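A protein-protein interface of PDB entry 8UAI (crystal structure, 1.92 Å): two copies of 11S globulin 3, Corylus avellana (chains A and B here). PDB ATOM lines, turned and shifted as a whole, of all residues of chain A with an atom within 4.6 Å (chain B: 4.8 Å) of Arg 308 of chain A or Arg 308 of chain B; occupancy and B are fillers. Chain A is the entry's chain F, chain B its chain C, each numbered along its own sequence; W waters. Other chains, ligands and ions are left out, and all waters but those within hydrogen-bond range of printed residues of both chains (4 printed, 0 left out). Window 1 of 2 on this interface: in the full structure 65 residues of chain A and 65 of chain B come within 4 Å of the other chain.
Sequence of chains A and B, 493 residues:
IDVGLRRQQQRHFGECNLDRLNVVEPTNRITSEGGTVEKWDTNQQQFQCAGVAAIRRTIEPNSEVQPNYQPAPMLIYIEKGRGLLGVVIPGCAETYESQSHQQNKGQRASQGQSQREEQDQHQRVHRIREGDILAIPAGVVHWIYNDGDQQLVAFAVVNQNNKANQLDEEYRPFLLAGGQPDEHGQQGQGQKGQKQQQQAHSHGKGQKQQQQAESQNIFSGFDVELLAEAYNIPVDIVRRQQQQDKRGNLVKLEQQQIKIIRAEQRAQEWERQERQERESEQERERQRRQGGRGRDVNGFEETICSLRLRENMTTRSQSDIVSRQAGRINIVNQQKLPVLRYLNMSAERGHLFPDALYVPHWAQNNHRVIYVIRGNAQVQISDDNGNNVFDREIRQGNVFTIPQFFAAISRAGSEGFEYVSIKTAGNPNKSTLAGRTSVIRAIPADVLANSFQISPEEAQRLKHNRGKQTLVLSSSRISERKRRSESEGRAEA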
ATOM      1  N   ARG A 124      13.383  14.506 -26.411  1.00  0.00           N
ATOM      2  CA  ARG A 124      13.588  15.868 -25.950  1.00  0.00           C
ATOM      3  C   ARG A 124      13.742  16.836 -27.124  1.00  0.00           C
ATOM      4  O   ARG A 124      14.205  16.476 -28.208  1.00  0.00           O
ATOM      5  CB  ARG A 124      14.776  15.940 -24.997  1.00  0.00           C
ATOM      6  CG  ARG A 124      16.090  15.932 -25.614  1.00  0.00           C
ATOM      7  CD  ARG A 124      17.149  15.753 -24.539  1.00  0.00           C
ATOM      8  NE  ARG A 124      18.204  14.922 -25.079  1.00  0.00           N
ATOM      9  CZ  ARG A 124      19.492  15.240 -25.111  1.00  0.00           C
ATOM     10  NH1 ARG A 124      19.961  16.304 -24.479  1.00  0.00           N
ATOM     11  NH2 ARG A 124      20.322  14.478 -25.808  1.00  0.00           N
ATOM     12  N   SER A 306      21.426  11.377 -22.847  1.00  0.00           N
ATOM     13  CA  SER A 306      21.606  12.682 -22.208  1.00  0.00           C
ATOM     14  C   SER A 306      22.677  13.516 -22.900  1.00  0.00           C
ATOM     15  O   SER A 306      23.153  14.509 -22.341  1.00  0.00           O
ATOM     16  CB  SER A 306      21.963  12.513 -20.735  1.00  0.00           C
ATOM     17  OG  SER A 306      23.214  11.860 -20.613  1.00  0.00           O
ATOM     18  N   LEU A 307      23.057  13.124 -24.104  1.00  0.00           N
ATOM     19  CA  LEU A 307      24.118  13.786 -24.839  1.00  0.00           C
ATOM     20  C   LEU A 307      23.707  15.188 -25.274  1.00  0.00           C
ATOM     21  O   LEU A 307      22.652  15.368 -25.885  1.00  0.00           O
ATOM     22  CB  LEU A 307      24.446  12.929 -26.047  1.00  0.00           C
ATOM     23  CG  LEU A 307      25.452  13.575 -26.932  1.00  0.00           C
ATOM     24  CD1 LEU A 307      26.561  13.931 -26.020  1.00  0.00           C
ATOM     25  CD2 LEU A 307      25.869  12.440 -27.859  1.00  0.00           C
ATOM     26  N   ARG A 308      24.549  16.188 -24.992  1.00  0.00           N
ATOM     27  CA  ARG A 308      24.181  17.553 -25.337  1.00  0.00           C
ATOM     28  C   ARG A 308      24.534  17.810 -26.801  1.00  0.00           C
ATOM     29  O   ARG A 308      25.556  17.341 -27.306  1.00  0.00           O
ATOM     30  CB  ARG A 308      24.842  18.548 -24.374  1.00  0.00           C
ATOM     31  CG  ARG A 308      25.124  19.934 -24.890  1.00  0.00           C
ATOM     32  CD  ARG A 308      25.801  20.739 -23.743  1.00  0.00           C
ATOM     33  NE  ARG A 308      25.223  22.074 -23.623  1.00  0.00           N
ATOM     34  CZ  ARG A 308      25.853  23.179 -24.011  1.00  0.00           C
ATOM     35  NH1 ARG A 308      27.134  23.156 -24.339  1.00  0.00           N
ATOM     36  NH2 ARG A 308      25.189  24.334 -24.051  1.00  0.00           N
ATOM     37  N   LEU A 309      23.641  18.505 -27.507  1.00  0.00           N
ATOM     38  CA  LEU A 309      23.681  18.617 -28.956  1.00  0.00           C
ATOM     39  C   LEU A 309      23.831  20.048 -29.448  1.00  0.00           C
ATOM     40  O   LEU A 309      24.012  20.254 -30.655  1.00  0.00           O
ATOM     41  CB  LEU A 309      22.401  18.025 -29.570  1.00  0.00           C
ATOM     42  CG  LEU A 309      22.089  16.546 -29.332  1.00  0.00           C
ATOM     43  CD1 LEU A 309      20.785  16.177 -30.031  1.00  0.00           C
ATOM     44  CD2 LEU A 309      23.207  15.654 -29.811  1.00  0.00           C
ATOM     45  N   ARG A 310      23.709  21.038 -28.569  1.00  0.00           N
ATOM     46  CA  ARG A 310      23.806  22.432 -28.976  1.00  0.00           C
ATOM     47  C   ARG A 310      24.769  23.148 -28.045  1.00  0.00           C
ATOM     48  O   ARG A 310      24.973  22.736 -26.898  1.00  0.00           O
ATOM     49  CB  ARG A 310      22.415  23.107 -28.977  1.00  0.00           C
ATOM     50  CG  ARG A 310      21.777  23.192 -27.621  1.00  0.00           C
ATOM     51  CD  ARG A 310      20.680  24.253 -27.629  1.00  0.00           C
ATOM     52  NE  ARG A 310      21.225  25.568 -27.304  1.00  0.00           N
ATOM     53  CZ  ARG A 310      21.851  25.863 -26.172  1.00  0.00           C
ATOM     54  NH1 ARG A 310      21.972  24.974 -25.197  1.00  0.00           N
ATOM     55  NH2 ARG A 310      22.370  27.079 -26.014  1.00  0.00           N
ATOM     56  N   GLU A 311      25.390  24.208 -28.555  1.00  0.00           N
ATOM     57  CA  GLU A 311      26.311  24.994 -27.749  1.00  0.00           C
ATOM     58  C   GLU A 311      26.301  26.404 -28.317  1.00  0.00           C
ATOM     59  O   GLU A 311      26.352  26.580 -29.536  1.00  0.00           O
ATOM     60  CB  GLU A 311      27.743  24.418 -27.779  1.00  0.00           C
ATOM     61  CG  GLU A 311      28.547  24.514 -26.453  1.00  0.00           C
ATOM     62  CD  GLU A 311      29.597  25.602 -26.427  1.00  0.00           C
ATOM     63  OE1 GLU A 311      29.843  26.217 -27.465  1.00  0.00           O
ATOM     64  OE2 GLU A 311      30.203  25.830 -25.359  1.00  0.00           O
ATOM     65  N   GLN A 318      32.090  33.144 -24.046  1.00  0.00           N
ATOM     66  CA  GLN A 318      33.192  32.202 -23.887  1.00  0.00           C
ATOM     67  C   GLN A 318      34.201  32.397 -25.011  1.00  0.00           C
ATOM     68  O   GLN A 318      33.835  32.363 -26.192  1.00  0.00           O
ATOM     69  CB  GLN A 318      32.690  30.744 -23.911  1.00  0.00           C
ATOM     70  CG  GLN A 318      32.236  30.170 -22.561  1.00  0.00           C
ATOM     71  CD  GLN A 318      31.616  28.773 -22.712  1.00  0.00           C
ATOM     72  OE1 GLN A 318      32.267  27.840 -23.188  1.00  0.00           O
ATOM     73  NE2 GLN A 318      30.370  28.626 -22.290  1.00  0.00           N
ATOM     74  N   GLN A 335      36.455  19.021 -26.386  1.00  0.00           N
ATOM     75  CA  GLN A 335      36.704  19.327 -24.987  1.00  0.00           C
ATOM     76  C   GLN A 335      35.756  20.407 -24.472  1.00  0.00           C
ATOM     77  O   GLN A 335      35.814  20.771 -23.288  1.00  0.00           O
ATOM     78  CB  GLN A 335      38.168  19.721 -24.800  1.00  0.00           C
ATOM     79  CG  GLN A 335      39.035  18.471 -24.513  1.00  0.00           C
ATOM     80  CD  GLN A 335      39.918  18.085 -25.658  1.00  0.00           C
ATOM     81  OE1 GLN A 335      40.289  18.922 -26.485  1.00  0.00           O
ATOM     82  NE2 GLN A 335      40.246  16.806 -25.740  1.00  0.00           N
ATOM     83  N   LYS A 336      34.879  20.903 -25.338  1.00  0.00           N
ATOM     84  CA  LYS A 336      33.748  21.741 -24.954  1.00  0.00           C
ATOM     85  C   LYS A 336      32.412  21.046 -25.136  1.00  0.00           C
ATOM     86  O   LYS A 336      31.501  21.249 -24.325  1.00  0.00           O
ATOM     87  CB  LYS A 336      33.728  23.040 -25.778  1.00  0.00           C
ATOM     88  CG  LYS A 336      35.005  23.896 -25.686  1.00  0.00           C
ATOM     89  CD  LYS A 336      34.646  25.364 -25.621  1.00  0.00           C
ATOM     90  CE  LYS A 336      35.791  26.199 -25.080  1.00  0.00           C
ATOM     91  NZ  LYS A 336      37.112  25.820 -25.670  1.00  0.00           N
ATOM     92  N   LEU A 337      32.261  20.277 -26.214  1.00  0.00           N
ATOM     93  CA  LEU A 337      30.996  19.636 -26.568  1.00  0.00           C
ATOM     94  C   LEU A 337      31.292  18.168 -26.847  1.00  0.00           C
ATOM     95  O   LEU A 337      31.806  17.827 -27.930  1.00  0.00           O
ATOM     96  CB  LEU A 337      30.354  20.334 -27.767  1.00  0.00           C
ATOM     97  CG  LEU A 337      29.030  19.758 -28.245  1.00  0.00           C
ATOM     98  CD1 LEU A 337      28.040  19.772 -27.087  1.00  0.00           C
ATOM     99  CD2 LEU A 337      28.486  20.576 -29.425  1.00  0.00           C
ATOM    100  N   VAL A 339      30.000  15.295 -27.763  1.00  0.00           N
ATOM    101  CA  VAL A 339      29.603  14.471 -28.901  1.00  0.00           C
ATOM    102  C   VAL A 339      30.442  14.748 -30.132  1.00  0.00           C
ATOM    103  O   VAL A 339      30.447  13.935 -31.062  1.00  0.00           O
ATOM    104  CB  VAL A 339      28.112  14.659 -29.229  1.00  0.00           C
ATOM    105  CG1 VAL A 339      27.841  16.024 -29.861  1.00  0.00           C
ATOM    106  CG2 VAL A 339      27.621  13.464 -30.124  1.00  0.00           C
ATOM    107  N   ARG B 124      43.023  32.306 -19.405  1.00  0.00           N
ATOM    108  CA  ARG B 124      41.603  32.497 -19.663  1.00  0.00           C
ATOM    109  C   ARG B 124      40.814  32.735 -18.371  1.00  0.00           C
ATOM    110  O   ARG B 124      41.061  32.092 -17.348  1.00  0.00           O
ATOM    111  CB  ARG B 124      41.109  31.243 -20.402  1.00  0.00           C
ATOM    112  CG  ARG B 124      39.624  31.066 -20.581  1.00  0.00           C
ATOM    113  CD  ARG B 124      39.410  29.857 -21.501  1.00  0.00           C
ATOM    114  NE  ARG B 124      40.022  28.653 -20.943  1.00  0.00           N
ATOM    115  CZ  ARG B 124      39.471  27.449 -20.988  1.00  0.00           C
ATOM    116  NH1 ARG B 124      38.347  27.232 -21.654  1.00  0.00           N
ATOM    117  NH2 ARG B 124      40.053  26.444 -20.339  1.00  0.00           N
ATOM    118  N   SER B 306      41.885  24.100 -23.854  1.00  0.00           N
ATOM    119  CA  SER B 306      40.593  24.513 -24.387  1.00  0.00           C
ATOM    120  C   SER B 306      39.410  23.861 -23.671  1.00  0.00           C
ATOM    121  O   SER B 306      38.292  23.899 -24.196  1.00  0.00           O
ATOM    122  CB  SER B 306      40.516  24.173 -25.879  1.00  0.00           C
ATOM    123  OG  SER B 306      41.438  24.952 -26.639  1.00  0.00           O
ATOM    124  N   LEU B 307      39.630  23.272 -22.498  1.00  0.00           N
ATOM    125  CA  LEU B 307      38.569  22.553 -21.807  1.00  0.00           C
ATOM    126  C   LEU B 307      37.518  23.509 -21.244  1.00  0.00           C
ATOM    127  O   LEU B 307      37.843  24.568 -20.700  1.00  0.00           O
ATOM    128  CB  LEU B 307      39.177  21.726 -20.685  1.00  0.00           C
ATOM    129  CG  LEU B 307      38.226  20.827 -19.931  1.00  0.00           C
ATOM    130  CD1 LEU B 307      37.485  19.949 -20.894  1.00  0.00           C
ATOM    131  CD2 LEU B 307      39.083  19.998 -19.013  1.00  0.00           C
ATOM    132  N   ARG B 308      36.252  23.126 -21.359  1.00  0.00           N
ATOM    133  CA  ARG B 308      35.179  23.928 -20.785  1.00  0.00           C
ATOM    134  C   ARG B 308      35.054  23.599 -19.304  1.00  0.00           C
ATOM    135  O   ARG B 308      35.079  22.430 -18.928  1.00  0.00           O
ATOM    136  CB  ARG B 308      33.865  23.647 -21.507  1.00  0.00           C
ATOM    137  CG  ARG B 308      32.705  24.546 -21.127  1.00  0.00           C
ATOM    138  CD  ARG B 308      31.616  24.374 -22.167  1.00  0.00           C
ATOM    139  NE  ARG B 308      30.610  25.415 -22.057  1.00  0.00           N
ATOM    140  CZ  ARG B 308      29.350  25.175 -21.721  1.00  0.00           C
ATOM    141  NH1 ARG B 308      28.931  23.939 -21.448  1.00  0.00           N
ATOM    142  NH2 ARG B 308      28.495  26.193 -21.650  1.00  0.00           N
ATOM    143  N   LEU B 309      34.931  24.619 -18.454  1.00  0.00           N
ATOM    144  CA  LEU B 309      34.796  24.327 -17.033  1.00  0.00           C
ATOM    145  C   LEU B 309      33.507  24.854 -16.417  1.00  0.00           C
ATOM    146  O   LEU B 309      33.289  24.641 -15.224  1.00  0.00           O
ATOM    147  CB  LEU B 309      36.003  24.871 -16.252  1.00  0.00           C
ATOM    148  CG  LEU B 309      36.031  26.329 -15.834  1.00  0.00           C
ATOM    149  CD1 LEU B 309      35.656  26.379 -14.364  1.00  0.00           C
ATOM    150  CD2 LEU B 309      37.403  26.893 -16.024  1.00  0.00           C
ATOM    151  N   ARG B 310      32.649  25.503 -17.187  1.00  0.00           N
ATOM    152  CA  ARG B 310      31.365  25.984 -16.680  1.00  0.00           C
ATOM    153  C   ARG B 310      30.238  25.468 -17.566  1.00  0.00           C
ATOM    154  O   ARG B 310      30.432  25.214 -18.754  1.00  0.00           O
ATOM    155  CB  ARG B 310      31.338  27.519 -16.613  1.00  0.00           C
ATOM    156  CG  ARG B 310      31.371  28.173 -17.981  1.00  0.00           C
ATOM    157  CD  ARG B 310      30.856  29.591 -17.914  1.00  0.00           C
ATOM    158  NE  ARG B 310      29.418  29.604 -17.687  1.00  0.00           N
ATOM    159  CZ  ARG B 310      28.503  29.564 -18.648  1.00  0.00           C
ATOM    160  NH1 ARG B 310      28.839  29.426 -19.920  1.00  0.00           N
ATOM    161  NH2 ARG B 310      27.216  29.657 -18.321  1.00  0.00           N
ATOM    162  N   GLU B 311      29.067  25.268 -16.964  1.00  0.00           N
ATOM    163  CA  GLU B 311      27.868  24.868 -17.688  1.00  0.00           C
ATOM    164  C   GLU B 311      26.655  25.382 -16.914  1.00  0.00           C
ATOM    165  O   GLU B 311      26.590  25.218 -15.692  1.00  0.00           O
ATOM    166  CB  GLU B 311      27.809  23.339 -17.859  1.00  0.00           C
ATOM    167  CG  GLU B 311      26.402  22.784 -17.888  1.00  0.00           C
ATOM    168  CD  GLU B 311      25.869  22.611 -19.281  1.00  0.00           C
ATOM    169  OE1 GLU B 311      26.576  22.988 -20.243  1.00  0.00           O
ATOM    170  OE2 GLU B 311      24.714  22.154 -19.410  1.00  0.00           O
ATOM    171  N   GLN B 318      17.837  23.898 -20.659  1.00  0.00           N
ATOM    172  CA  GLN B 318      17.988  22.522 -21.128  1.00  0.00           C
ATOM    173  C   GLN B 318      17.431  21.571 -20.086  1.00  0.00           C
ATOM    174  O   GLN B 318      17.666  21.754 -18.888  1.00  0.00           O
ATOM    175  CB  GLN B 318      19.450  22.109 -21.400  1.00  0.00           C
ATOM    176  CG  GLN B 318      20.240  22.942 -22.401  1.00  0.00           C
ATOM    177  CD  GLN B 318      21.755  22.785 -22.221  1.00  0.00           C
ATOM    178  OE1 GLN B 318      22.324  21.732 -22.537  1.00  0.00           O
ATOM    179  NE2 GLN B 318      22.417  23.850 -21.762  1.00  0.00           N
ATOM    180  N   GLN B 335      28.544  13.555 -20.506  1.00  0.00           N
ATOM    181  CA  GLN B 335      28.031  13.667 -21.870  1.00  0.00           C
ATOM    182  C   GLN B 335      27.536  15.070 -22.207  1.00  0.00           C
ATOM    183  O   GLN B 335      27.111  15.315 -23.345  1.00  0.00           O
ATOM    184  CB  GLN B 335      26.927  12.654 -22.114  1.00  0.00           C
ATOM    185  CG  GLN B 335      27.434  11.519 -22.952  1.00  0.00           C
ATOM    186  CD  GLN B 335      27.998  10.429 -22.092  1.00  0.00           C
ATOM    187  OE1 GLN B 335      27.490  10.152 -21.002  1.00  0.00           O
ATOM    188  NE2 GLN B 335      29.085   9.839 -22.540  1.00  0.00           N
ATOM    189  N   LYS B 336      27.599  15.985 -21.253  1.00  0.00           N
ATOM    190  CA  LYS B 336      27.339  17.392 -21.491  1.00  0.00           C
ATOM    191  C   LYS B 336      28.546  18.273 -21.227  1.00  0.00           C
ATOM    192  O   LYS B 336      28.706  19.289 -21.907  1.00  0.00           O
ATOM    193  CB  LYS B 336      26.172  17.869 -20.613  1.00  0.00           C
ATOM    194  CG  LYS B 336      24.842  17.086 -20.812  1.00  0.00           C
ATOM    195  CD  LYS B 336      23.630  17.913 -20.367  1.00  0.00           C
ATOM    196  CE  LYS B 336      22.316  17.418 -20.961  1.00  0.00           C
ATOM    197  NZ  LYS B 336      22.001  16.030 -20.510  1.00  0.00           N
ATOM    198  N   LEU B 337      29.386  17.916 -20.259  1.00  0.00           N
ATOM    199  CA  LEU B 337      30.574  18.686 -19.883  1.00  0.00           C
ATOM    200  C   LEU B 337      31.771  17.738 -19.811  1.00  0.00           C
ATOM    201  O   LEU B 337      31.966  17.051 -18.793  1.00  0.00           O
ATOM    202  CB  LEU B 337      30.355  19.397 -18.553  1.00  0.00           C
ATOM    203  CG  LEU B 337      31.432  20.420 -18.178  1.00  0.00           C
ATOM    204  CD1 LEU B 337      31.561  21.500 -19.260  1.00  0.00           C
ATOM    205  CD2 LEU B 337      31.090  21.068 -16.849  1.00  0.00           C
ATOM    206  N   VAL B 339      34.937  17.499 -19.139  1.00  0.00           N
ATOM    207  CA  VAL B 339      35.927  17.368 -18.073  1.00  0.00           C
ATOM    208  C   VAL B 339      35.414  16.544 -16.899  1.00  0.00           C
ATOM    209  O   VAL B 339      36.211  16.024 -16.113  1.00  0.00           O
ATOM    210  CB  VAL B 339      36.409  18.777 -17.637  1.00  0.00           C
ATOM    211  CG1 VAL B 339      35.321  19.523 -16.880  1.00  0.00           C
ATOM    212  CG2 VAL B 339      37.683  18.674 -16.790  1.00  0.00           C
HETATM  213  O   HOH W   1      27.744  16.407 -26.415  1.00  0.00           O
HETATM  214  O   HOH W   2      29.027  21.784 -23.398  1.00  0.00           O
HETATM  215  O   HOH W   3      34.774  20.150 -20.362  1.00  0.00           O
HETATM  216  O   HOH W   4      26.423  26.921 -24.369  1.00  0.00           O
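The side-chain amino group (NZ) of Lys 336 of chain A lies within hydrogen-bond range of the backbone carbonyl oxygen (O) of Ser 306 of chain B (2.7 Å). The guanidinium group (NE) of Arg 308 of chain B lies within salt-bridge range of the side-chain carboxylate (OE2) of Glu 311 of chain A, at 3.4 Å. The guanidinium group of Arg 308 of chain B lies close to the side-chain amide nitrogen of Gln 318 of chain A, at 3.1 Å. The backbone NH of Arg 308 of chain B sits at hydrogen-bond distance from the backbone carbonyl oxygen of Gln 335 of chain A. The guanidinium group of Arg 310 of chain B lies close to the side-chain amide nitrogen of Gln 318 of chain A (2.9 Å). The guanidinium group (NE) of Arg 308 of chain A lies within salt-bridge range of the side-chain carboxylate (OE1) of Glu 311 of chain B, 3.8 Å away. The side-chain amide oxygen of Gln 318 of chain B is in hydrogen-bond range of the guanidinium group of Arg 308 of chain A (3.1 Å). The backbone NH (N) of Arg 308 of chain A is in hydrogen-bond range of the backbone carbonyl oxygen (O) of Gln 335 of chain B, 3.2 Å away. NZ of Lys 336 of chain B lies within hydrogen-bond range of O of Ser 306 of chain A, at 2.6 Å. The guanidinium group (NH1) of Arg 308 of chain B sits close to the guanidinium group (NH1) of Arg 308 of chain A, at 3.5 Å.
O of Leu 307 of chain B sits at hydrogen-bond distance from NH1 of Arg 124 of chain B. NE of Arg 308 of chain B sits close to O of Arg 310 of chain B, at 3.3 Å. The guanidinium group (NH1) of Arg 308 of chain B lies within salt-bridge range of the side-chain carboxylate (OE1) of Glu 311 of chain B (2.8 Å). The guanidinium group of Arg 124 of chain A is in hydrogen-bond range of the backbone carbonyl oxygen of Leu 307 of chain A, at 2.5 Å. The guanidinium group (NH2) of Arg 308 of chain A lies close to the backbone carbonyl oxygen (O) of Arg 310 of chain A (3.3 Å).
Leu 307 of chain A touches Gln 335 of chain B (CD1 to O, 3.1 Å). Arg 308 of chain A touches Lys 336 of chain B. Arg 310 of chain A touches Gln 318 of chain B (NH1 to NE2, 3.6 Å). Gln 335 of chain A touches Leu 307 of chain B. O of Lys 336 of chain A touches CD of Arg 308 of chain B, 3.8 Å away.
Of chain B, only Arg 308, Glu 311, Gln 318, Gln 335 and Lys 336 come within 4 Å of Arg 308 of chain A. Of the printed residues of chain B, Glu 311 of chain A touches Arg 308 (3.4 Å). Of the printed residues of chain A, Gln 335 of chain B touches Leu 307 (3.1 Å) and Arg 308 (3.2 Å). Printed residues of chain A within 4 Å of Glu 311 of chain B: Arg 308 (3.8 Å). Of the printed residues of chain B, Lys 336 of chain A touches Ser 306 and Arg 308. Printed residues of chain A within 4 Å of Gln 318 of chain B: Arg 308 and Arg 310. The nearest printed residue of chain A that does not touch Arg 308 of chain B is Leu 337 of chain A (5.8 Å). The nearest printed residue of chain B that does not touch Lys 336 of chain A is Lys 336 of chain B (4.2 Å).
Of the 12 printed residues of chain A, 8 touch a printed residue of chain B. Printed residues of chain A that touch a printed residue of chain B: Ser 306, Leu 307, Arg 308, Arg 310, Glu 311, Gln 318, Gln 335 and Lys 336. Hydrophobic or aromatic side chains of chain A within 4 Å of the printed part of chain B: Leu 307. Of the 12 printed residues of chain B, 8 touch a printed residue of chain A. Among the printed residues, 15 pairs touch across the chains.
Ser 306 of chain A touches Lys 336 of chain B, and with the chains exchanged Lys 336 of chain A touches Ser 306 of chain B. Arg 308 of chain A touches Glu 311 of chain B, and with the chains exchanged Glu 311 of chain A touches Arg 308 of chain B. Arg 308 of chain A touches Gln 335 of chain B, and with the chains exchanged Gln 335 of chain A touches Arg 308 of chain B. Arg 308 of chain A touches Lys 336 of chain B, and with the chains exchanged Lys 336 of chain A touches Arg 308 of chain B. 12 positions are printed for both chains.
Water W2 lies within hydrogen-bond range of the guanidinium group (NH1) of Arg 308 of chain A (2.5 Å), the backbone carbonyl oxygen (O) of Lys 336 of chain A (2.7 Å), the guanidinium group (NH1) of Arg 308 of chain B (2.9 Å) and the backbone carbonyl oxygen (O) of Lys 336 of chain B (2.9 Å). Water W1 lies within hydrogen-bond range of the backbone carbonyl oxygen (O) of Arg 308 of chain A (2.5 Å), the backbone NH (N) of Val 339 of chain A (2.9 Å) and the backbone carbonyl oxygen (O) of Gln 335 of chain B (3.3 Å). Water W3 lies within hydrogen-bond range of the backbone carbonyl oxygen (O) of Arg 308 of chain B, the backbone NH (N) of Val 339 of chain B and the backbone carbonyl oxygen (O) of Gln 335 of chain A. Water W4 lies within hydrogen-bond range of the guanidinium group of Arg 308 of chain A and the guanidinium group of Arg 308 of chain B.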
